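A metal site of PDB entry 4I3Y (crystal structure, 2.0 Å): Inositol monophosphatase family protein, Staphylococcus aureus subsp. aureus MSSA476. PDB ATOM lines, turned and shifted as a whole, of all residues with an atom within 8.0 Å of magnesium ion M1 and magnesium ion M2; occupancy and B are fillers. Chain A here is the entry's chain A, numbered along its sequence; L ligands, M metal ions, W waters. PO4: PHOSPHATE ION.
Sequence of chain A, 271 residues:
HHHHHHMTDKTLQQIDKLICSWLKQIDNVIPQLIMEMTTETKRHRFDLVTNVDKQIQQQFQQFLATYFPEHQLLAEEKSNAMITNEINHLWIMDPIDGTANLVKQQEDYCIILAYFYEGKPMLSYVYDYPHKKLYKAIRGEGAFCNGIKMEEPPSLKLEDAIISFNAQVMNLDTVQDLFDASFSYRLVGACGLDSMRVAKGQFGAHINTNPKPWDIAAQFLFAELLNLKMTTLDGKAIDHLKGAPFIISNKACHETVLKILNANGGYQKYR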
ATOM      1  N   LYS A  42       7.957  15.048  27.336  1.00  0.00           N
ATOM      2  CA  LYS A  42       7.689  16.157  26.406  1.00  0.00           C
ATOM      3  C   LYS A  42       6.325  15.888  25.770  1.00  0.00           C
ATOM      4  O   LYS A  42       5.320  16.179  26.382  1.00  0.00           O
ATOM      5  CB  LYS A  42       8.830  16.343  25.367  1.00  0.00           C
ATOM      6  CG  LYS A  42      10.216  16.588  25.988  1.00  0.00           C
ATOM      7  CD  LYS A  42      11.215  17.080  24.952  1.00  0.00           C
ATOM      8  CE  LYS A  42      11.785  15.924  24.162  1.00  0.00           C
ATOM      9  NZ  LYS A  42      12.732  16.410  23.144  1.00  0.00           N
ATOM     10  N   PHE A  46       6.216   8.686  27.324  1.00  0.00           N
ATOM     11  CA  PHE A  46       7.388   7.914  26.855  1.00  0.00           C
ATOM     12  C   PHE A  46       8.377   8.774  26.010  1.00  0.00           C
ATOM     13  O   PHE A  46       9.406   8.267  25.564  1.00  0.00           O
ATOM     14  CB  PHE A  46       6.915   6.733  25.943  1.00  0.00           C
ATOM     15  CG  PHE A  46       6.004   5.748  26.628  1.00  0.00           C
ATOM     16  CD1 PHE A  46       6.508   4.493  27.071  1.00  0.00           C
ATOM     17  CD2 PHE A  46       4.643   6.017  26.811  1.00  0.00           C
ATOM     18  CE1 PHE A  46       5.699   3.561  27.714  1.00  0.00           C
ATOM     19  CE2 PHE A  46       3.824   5.078  27.460  1.00  0.00           C
ATOM     20  CZ  PHE A  46       4.357   3.847  27.909  1.00  0.00           C
ATOM     21  N   ASP A  47       8.056  10.052  25.766  1.00  0.00           N
ATOM     22  CA  ASP A  47       8.947  10.919  25.019  1.00  0.00           C
ATOM     23  C   ASP A  47       9.873  11.630  26.012  1.00  0.00           C
ATOM     24  O   ASP A  47       9.554  12.747  26.442  1.00  0.00           O
ATOM     25  CB  ASP A  47       8.143  11.960  24.283  1.00  0.00           C
ATOM     26  CG  ASP A  47       8.982  12.776  23.324  1.00  0.00           C
ATOM     27  OD1 ASP A  47      10.122  12.331  22.978  1.00  0.00           O
ATOM     28  OD2 ASP A  47       8.514  13.834  22.902  1.00  0.00           O
ATOM     29  N   LEU A  48      11.014  11.024  26.340  1.00  0.00           N
ATOM     30  CA  LEU A  48      11.837  11.419  27.520  1.00  0.00           C
ATOM     31  C   LEU A  48      12.934  12.468  27.236  1.00  0.00           C
ATOM     32  O   LEU A  48      13.463  12.535  26.128  1.00  0.00           O
ATOM     33  CB  LEU A  48      12.502  10.176  28.090  1.00  0.00           C
ATOM     34  CG  LEU A  48      11.791   9.399  29.183  1.00  0.00           C
ATOM     35  CD1 LEU A  48      10.298   9.505  29.093  1.00  0.00           C
ATOM     36  CD2 LEU A  48      12.277   7.957  29.317  1.00  0.00           C
ATOM     37  N   VAL A  49      13.284  13.255  28.252  1.00  0.00           N
ATOM     38  CA  VAL A  49      14.446  14.154  28.222  1.00  0.00           C
ATOM     39  C   VAL A  49      15.055  14.191  29.613  1.00  0.00           C
ATOM     40  O   VAL A  49      14.324  14.123  30.611  1.00  0.00           O
ATOM     41  CB  VAL A  49      14.144  15.609  27.663  1.00  0.00           C
ATOM     42  CG1 VAL A  49      13.075  16.383  28.471  1.00  0.00           C
ATOM     43  CG2 VAL A  49      15.418  16.442  27.652  1.00  0.00           C
ATOM     44  N   THR A  50      16.385  14.152  29.693  1.00  0.00           N
ATOM     45  CA  THR A  50      16.989  14.180  31.028  1.00  0.00           C
ATOM     46  C   THR A  50      17.914  15.377  31.187  1.00  0.00           C
ATOM     47  O   THR A  50      18.131  16.144  30.246  1.00  0.00           O
ATOM     48  CB  THR A  50      17.820  12.911  31.293  1.00  0.00           C
ATOM     49  OG1 THR A  50      19.009  12.943  30.479  1.00  0.00           O
ATOM     50  CG2 THR A  50      16.969  11.616  31.006  1.00  0.00           C
ATOM     51  N   ASP A  53      20.763  15.055  28.640  1.00  0.00           N
ATOM     52  CA  ASP A  53      20.460  15.704  27.364  1.00  0.00           C
ATOM     53  C   ASP A  53      20.640  17.232  27.512  1.00  0.00           C
ATOM     54  O   ASP A  53      21.324  17.853  26.700  1.00  0.00           O
ATOM     55  CB  ASP A  53      18.991  15.462  26.902  1.00  0.00           C
ATOM     56  CG  ASP A  53      18.577  13.993  26.882  1.00  0.00           C
ATOM     57  OD1 ASP A  53      18.482  13.350  27.993  1.00  0.00           O
ATOM     58  OD2 ASP A  53      18.318  13.481  25.735  1.00  0.00           O
ATOM     59  N   GLN A  57      23.647  19.670  25.801  1.00  0.00           N
ATOM     60  CA  GLN A  57      23.258  20.662  24.792  1.00  0.00           C
ATOM     61  C   GLN A  57      23.747  22.061  25.160  1.00  0.00           C
ATOM     62  O   GLN A  57      24.266  22.820  24.341  1.00  0.00           O
ATOM     63  CB  GLN A  57      21.744  20.716  24.615  1.00  0.00           C
ATOM     64  CG  GLN A  57      21.404  21.616  23.432  1.00  0.00           C
ATOM     65  CD  GLN A  57      19.940  21.482  22.974  1.00  0.00           C
ATOM     66  OE1 GLN A  57      19.185  22.428  23.048  1.00  0.00           O
ATOM     67  NE2 GLN A  57      19.571  20.326  22.505  1.00  0.00           N
ATOM     68  N   ALA A  75      18.966  22.389  17.469  1.00  0.00           N
ATOM     69  CA  ALA A  75      19.151  21.284  18.435  1.00  0.00           C
ATOM     70  C   ALA A  75      17.850  20.843  19.084  1.00  0.00           C
ATOM     71  O   ALA A  75      16.896  21.660  19.314  1.00  0.00           O
ATOM     72  CB  ALA A  75      20.164  21.652  19.507  1.00  0.00           C
ATOM     73  N   GLU A  76      17.822  19.558  19.428  1.00  0.00           N
ATOM     74  CA  GLU A  76      16.634  18.969  19.989  1.00  0.00           C
ATOM     75  C   GLU A  76      15.976  19.677  21.204  1.00  0.00           C
ATOM     76  O   GLU A  76      14.750  19.923  21.229  1.00  0.00           O
ATOM     77  CB  GLU A  76      16.880  17.519  20.377  1.00  0.00           C
ATOM     78  CG  GLU A  76      15.555  16.881  20.797  1.00  0.00           C
ATOM     79  CD  GLU A  76      15.652  15.367  20.944  1.00  0.00           C
ATOM     80  OE1 GLU A  76      14.597  14.739  21.250  1.00  0.00           O
ATOM     81  OE2 GLU A  76      16.763  14.836  20.733  1.00  0.00           O
ATOM     82  N   GLU A  77      16.755  19.995  22.227  1.00  0.00           N
ATOM     83  CA  GLU A  77      16.136  20.414  23.471  1.00  0.00           C
ATOM     84  C   GLU A  77      15.974  21.955  23.622  1.00  0.00           C
ATOM     85  O   GLU A  77      16.109  22.479  24.684  1.00  0.00           O
ATOM     86  CB  GLU A  77      16.824  19.794  24.689  1.00  0.00           C
ATOM     87  CG  GLU A  77      17.213  18.312  24.555  1.00  0.00           C
ATOM     88  CD  GLU A  77      16.016  17.338  24.308  1.00  0.00           C
ATOM     89  OE1 GLU A  77      14.821  17.747  24.489  1.00  0.00           O
ATOM     90  OE2 GLU A  77      16.276  16.151  23.898  1.00  0.00           O
ATOM     91  N   MET A  93      22.470  19.523  16.345  1.00  0.00           N
ATOM     92  CA  MET A  93      22.876  18.642  17.459  1.00  0.00           C
ATOM     93  C   MET A  93      21.753  17.826  18.070  1.00  0.00           C
ATOM     94  O   MET A  93      20.726  18.376  18.473  1.00  0.00           O
ATOM     95  CB  MET A  93      23.516  19.423  18.610  1.00  0.00           C
ATOM     96  CG  MET A  93      23.974  18.569  19.796  1.00  0.00           C
ATOM     97  SD  MET A  93      24.577  19.593  21.170  1.00  0.00           S
ATOM     98  CE  MET A  93      25.896  18.560  21.742  1.00  0.00           C
ATOM     99  N   ASP A  94      22.011  16.520  18.241  1.00  0.00           N
ATOM    100  CA  ASP A  94      21.177  15.701  19.136  1.00  0.00           C
ATOM    101  C   ASP A  94      22.020  15.414  20.392  1.00  0.00           C
ATOM    102  O   ASP A  94      22.980  14.629  20.310  1.00  0.00           O
ATOM    103  CB  ASP A  94      20.831  14.396  18.448  1.00  0.00           C
ATOM    104  CG  ASP A  94      19.697  13.693  19.140  1.00  0.00           C
ATOM    105  OD1 ASP A  94      19.510  13.918  20.353  1.00  0.00           O
ATOM    106  OD2 ASP A  94      18.980  12.996  18.415  1.00  0.00           O
ATOM    107  N   PRO A  95      21.700  16.077  21.543  1.00  0.00           N
ATOM    108  CA  PRO A  95      22.673  15.935  22.615  1.00  0.00           C
ATOM    109  C   PRO A  95      22.721  14.532  23.186  1.00  0.00           C
ATOM    110  O   PRO A  95      23.802  14.058  23.581  1.00  0.00           O
ATOM    111  CB  PRO A  95      22.230  16.966  23.631  1.00  0.00           C
ATOM    112  CG  PRO A  95      20.718  17.143  23.369  1.00  0.00           C
ATOM    113  CD  PRO A  95      20.602  17.029  21.875  1.00  0.00           C
ATOM    114  N   ILE A  96      21.564  13.859  23.282  1.00  0.00           N
ATOM    115  CA  ILE A  96      21.602  12.420  23.506  1.00  0.00           C
ATOM    116  C   ILE A  96      20.614  11.810  22.483  1.00  0.00           C
ATOM    117  O   ILE A  96      19.434  12.104  22.534  1.00  0.00           O
ATOM    118  CB  ILE A  96      21.162  12.006  24.923  1.00  0.00           C
ATOM    119  CG1 ILE A  96      22.201  12.435  26.015  1.00  0.00           C
ATOM    120  CG2 ILE A  96      20.835  10.491  24.962  1.00  0.00           C
ATOM    121  CD1 ILE A  96      23.439  11.563  26.021  1.00  0.00           C
ATOM    122  N   ASP A  97      21.122  11.009  21.551  1.00  0.00           N
ATOM    123  CA  ASP A  97      20.249  10.326  20.630  1.00  0.00           C
ATOM    124  C   ASP A  97      20.084   8.922  21.226  1.00  0.00           C
ATOM    125  O   ASP A  97      21.056   8.304  21.548  1.00  0.00           O
ATOM    126  CB  ASP A  97      20.786  10.292  19.215  1.00  0.00           C
ATOM    127  CG  ASP A  97      19.870   9.429  18.298  1.00  0.00           C
ATOM    128  OD1 ASP A  97      18.677   9.782  18.230  1.00  0.00           O
ATOM    129  OD2 ASP A  97      20.359   8.469  17.671  1.00  0.00           O
ATOM    130  N   GLY A  98      18.843   8.446  21.397  1.00  0.00           N
ATOM    131  CA  GLY A  98      18.572   7.269  22.213  1.00  0.00           C
ATOM    132  C   GLY A  98      18.419   7.544  23.722  1.00  0.00           C
ATOM    133  O   GLY A  98      18.902   6.772  24.573  1.00  0.00           O
ATOM    134  N   THR A  99      17.717   8.629  24.059  1.00  0.00           N
ATOM    135  CA  THR A  99      17.391   8.944  25.453  1.00  0.00           C
ATOM    136  C   THR A  99      16.705   7.778  26.180  1.00  0.00           C
ATOM    137  O   THR A  99      16.971   7.534  27.351  1.00  0.00           O
ATOM    138  CB  THR A  99      16.541  10.248  25.533  1.00  0.00           C
ATOM    139  OG1 THR A  99      17.218  11.262  24.757  1.00  0.00           O
ATOM    140  CG2 THR A  99      16.439  10.737  26.940  1.00  0.00           C
ATOM    141  N   ALA A 100      15.805   7.053  25.487  1.00  0.00           N
ATOM    142  CA  ALA A 100      15.113   5.931  26.135  1.00  0.00           C
ATOM    143  C   ALA A 100      16.141   4.898  26.580  1.00  0.00           C
ATOM    144  O   ALA A 100      16.109   4.435  27.688  1.00  0.00           O
ATOM    145  CB  ALA A 100      14.005   5.316  25.225  1.00  0.00           C
ATOM    146  N   CYS A 110      24.055   7.852  21.913  1.00  0.00           N
ATOM    147  CA  CYS A 110      25.148   8.568  21.352  1.00  0.00           C
ATOM    148  C   CYS A 110      24.849  10.067  21.354  1.00  0.00           C
ATOM    149  O   CYS A 110      23.729  10.512  21.702  1.00  0.00           O
ATOM    150  CB  CYS A 110      25.386   8.059  19.888  1.00  0.00           C
ATOM    151  SG  CYS A 110      23.932   8.255  18.780  1.00  0.00           S
ATOM    152  N   ILE A 111      25.870  10.847  21.021  1.00  0.00           N
ATOM    153  CA  ILE A 111      25.709  12.269  20.840  1.00  0.00           C
ATOM    154  C   ILE A 111      25.902  12.498  19.338  1.00  0.00           C
ATOM    155  O   ILE A 111      26.863  11.974  18.752  1.00  0.00           O
ATOM    156  CB  ILE A 111      26.780  13.042  21.627  1.00  0.00           C
ATOM    157  CG1 ILE A 111      26.702  12.746  23.099  1.00  0.00           C
ATOM    158  CG2 ILE A 111      26.699  14.560  21.408  1.00  0.00           C
ATOM    159  CD1 ILE A 111      27.849  13.399  23.877  1.00  0.00           C
ATOM    160  N   ILE A 112      24.981  13.231  18.706  1.00  0.00           N
ATOM    161  CA  ILE A 112      25.074  13.537  17.291  1.00  0.00           C
ATOM    162  C   ILE A 112      25.402  15.029  16.989  1.00  0.00           C
ATOM    163  O   ILE A 112      24.697  15.974  17.435  1.00  0.00           O
ATOM    164  CB  ILE A 112      23.810  13.094  16.498  1.00  0.00           C
ATOM    165  CG1 ILE A 112      23.553  11.602  16.791  1.00  0.00           C
ATOM    166  CG2 ILE A 112      23.963  13.370  14.977  1.00  0.00           C
ATOM    167  CD1 ILE A 112      22.304  11.003  16.132  1.00  0.00           C
ATOM    168  N   LYS A 212      13.553  13.481  13.418  1.00  0.00           N
ATOM    169  CA  LYS A 212      13.784  14.922  13.469  1.00  0.00           C
ATOM    170  C   LYS A 212      15.102  15.223  12.794  1.00  0.00           C
ATOM    171  O   LYS A 212      15.907  14.299  12.591  1.00  0.00           O
ATOM    172  CB  LYS A 212      13.851  15.369  14.905  1.00  0.00           C
ATOM    173  CG  LYS A 212      12.500  15.146  15.585  1.00  0.00           C
ATOM    174  CD  LYS A 212      11.457  16.194  15.187  1.00  0.00           C
ATOM    175  CE  LYS A 212      10.033  15.670  15.054  1.00  0.00           C
ATOM    176  NZ  LYS A 212       9.866  14.264  15.550  1.00  0.00           N
ATOM    177  N   TRP A 214      17.858  16.476  13.880  1.00  0.00           N
ATOM    178  CA  TRP A 214      19.017  16.115  14.730  1.00  0.00           C
ATOM    179  C   TRP A 214      19.242  14.583  14.799  1.00  0.00           C
ATOM    180  O   TRP A 214      20.376  14.179  15.000  1.00  0.00           O
ATOM    181  CB  TRP A 214      18.880  16.744  16.126  1.00  0.00           C
ATOM    182  CG  TRP A 214      17.494  16.590  16.706  1.00  0.00           C
ATOM    183  CD1 TRP A 214      16.969  15.453  17.277  1.00  0.00           C
ATOM    184  CD2 TRP A 214      16.432  17.560  16.706  1.00  0.00           C
ATOM    185  NE1 TRP A 214      15.675  15.670  17.661  1.00  0.00           N
ATOM    186  CE2 TRP A 214      15.318  16.965  17.354  1.00  0.00           C
ATOM    187  CE3 TRP A 214      16.334  18.900  16.285  1.00  0.00           C
ATOM    188  CZ2 TRP A 214      14.089  17.646  17.581  1.00  0.00           C
ATOM    189  CZ3 TRP A 214      15.096  19.578  16.498  1.00  0.00           C
ATOM    190  CH2 TRP A 214      14.006  18.952  17.123  1.00  0.00           C
ATOM    191  N   ASP A 215      18.192  13.762  14.633  1.00  0.00           N
ATOM    192  CA  ASP A 215      18.379  12.272  14.655  1.00  0.00           C
ATOM    193  C   ASP A 215      19.179  11.762  13.442  1.00  0.00           C
ATOM    194  O   ASP A 215      19.759  10.668  13.498  1.00  0.00           O
ATOM    195  CB  ASP A 215      17.021  11.530  14.665  1.00  0.00           C
ATOM    196  CG  ASP A 215      16.130  11.926  15.802  1.00  0.00           C
ATOM    197  OD1 ASP A 215      16.545  11.940  16.994  1.00  0.00           O
ATOM    198  OD2 ASP A 215      14.961  12.221  15.472  1.00  0.00           O
HETATM  199  P   PO4 L   1      16.157  11.342  21.329  1.00  0.00           P
HETATM  200  O1  PO4 L   1      14.723  11.681  20.904  1.00  0.00           O
HETATM  201  O2  PO4 L   1      16.311   9.852  21.744  1.00  0.00           O
HETATM  202  O3  PO4 L   1      17.007  11.642  20.111  1.00  0.00           O
HETATM  203  O4  PO4 L   1      16.463  12.185  22.606  1.00  0.00           O
HETATM  204 MG    MG M   1      18.000  13.295  21.452  1.00  0.00          MG
HETATM  205 MG    MG M   2      14.179  12.938  22.435  1.00  0.00          MG
HETATM  206  O   HOH W   1      12.176  13.601  21.807  1.00  0.00           O
HETATM  207  O   HOH W   2      14.510  14.178  24.074  1.00  0.00           O
HETATM  208  O   HOH W   3      13.480  11.381  23.743  1.00  0.00           O
HETATM  209  O   HOH W   4      18.317  14.774  23.151  1.00  0.00           O
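The backbone carbonyl oxygen (O) of Ile 112 is in hydrogen-bond range of the backbone NH (N) of Asp 94, 2.9 Å away. The indole nitrogen (NE1) of Trp 214 lies close to the side-chain carboxylate (OE2) of Glu 76. The backbone carbonyl oxygen of Met 93 lies within hydrogen-bond range of the backbone NH of Glu 76 (3.3 Å). O of Ile 96 lies close to OG1 of Thr 99 (3.2 Å). N of Asp 97 is in hydrogen-bond range of O of Cys 110 (2.7 Å). NZ of Lys 42 lies within salt-bridge range of OE1 of Glu 77. N of Lys 42 sits at hydrogen-bond distance from O of Asp 47 (2.9 Å). OG1 of Thr 99 is in hydrogen-bond range of OD2 of Asp 53, 2.7 Å away.
Magnesium ion M2 is bound by an oxygen (O1) of the ligand, water W2, water W3, the side-chain carboxylate (OE1) of Glu 76, water W1 and an oxygen (O4) of the ligand. Magnesium ion M2 has six donor atoms within binding distance.
Magnesium ion M1 is bound by the side-chain carboxylate (OD1) of Asp 94, the side-chain carboxylate (OE2) of Glu 76, the backbone carbonyl oxygen (O) of Ile 96, an oxygen (O4) of the ligand, water W4 and an oxygen (O3) of the ligand.
Water W4 lies within hydrogen-bond range of the side-chain carboxylate of Glu 77 (2.6 Å), the side-chain carboxylate of Asp 53 (2.9 Å) and the backbone NH of Ile 96 (3.4 Å). Water W1 lies within hydrogen-bond range of the side-chain carboxylate (OD1) of Asp 47 (2.7 Å) and the side-chain amino group (NZ) of Lys 42 (3.2 Å). Water W2 lies within hydrogen-bond range of OE2 of Glu 77 (2.7 Å), O of Leu 48 (2.8 Å) and NZ of Lys 42 (3.0 Å).
Residues that only touch magnesium ion M1: Asp 97 (3.8 Å) and Thr 99 (3.96 Å).
NZ of Lys 42 touches magnesium ion M2, at 3.8 Å. O of Leu 48 touches magnesium ion M2, 3.8 Å away. Three residues have an atom within 4 Å of magnesium ion M2: Lys 42, Leu 48 and Glu 76.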
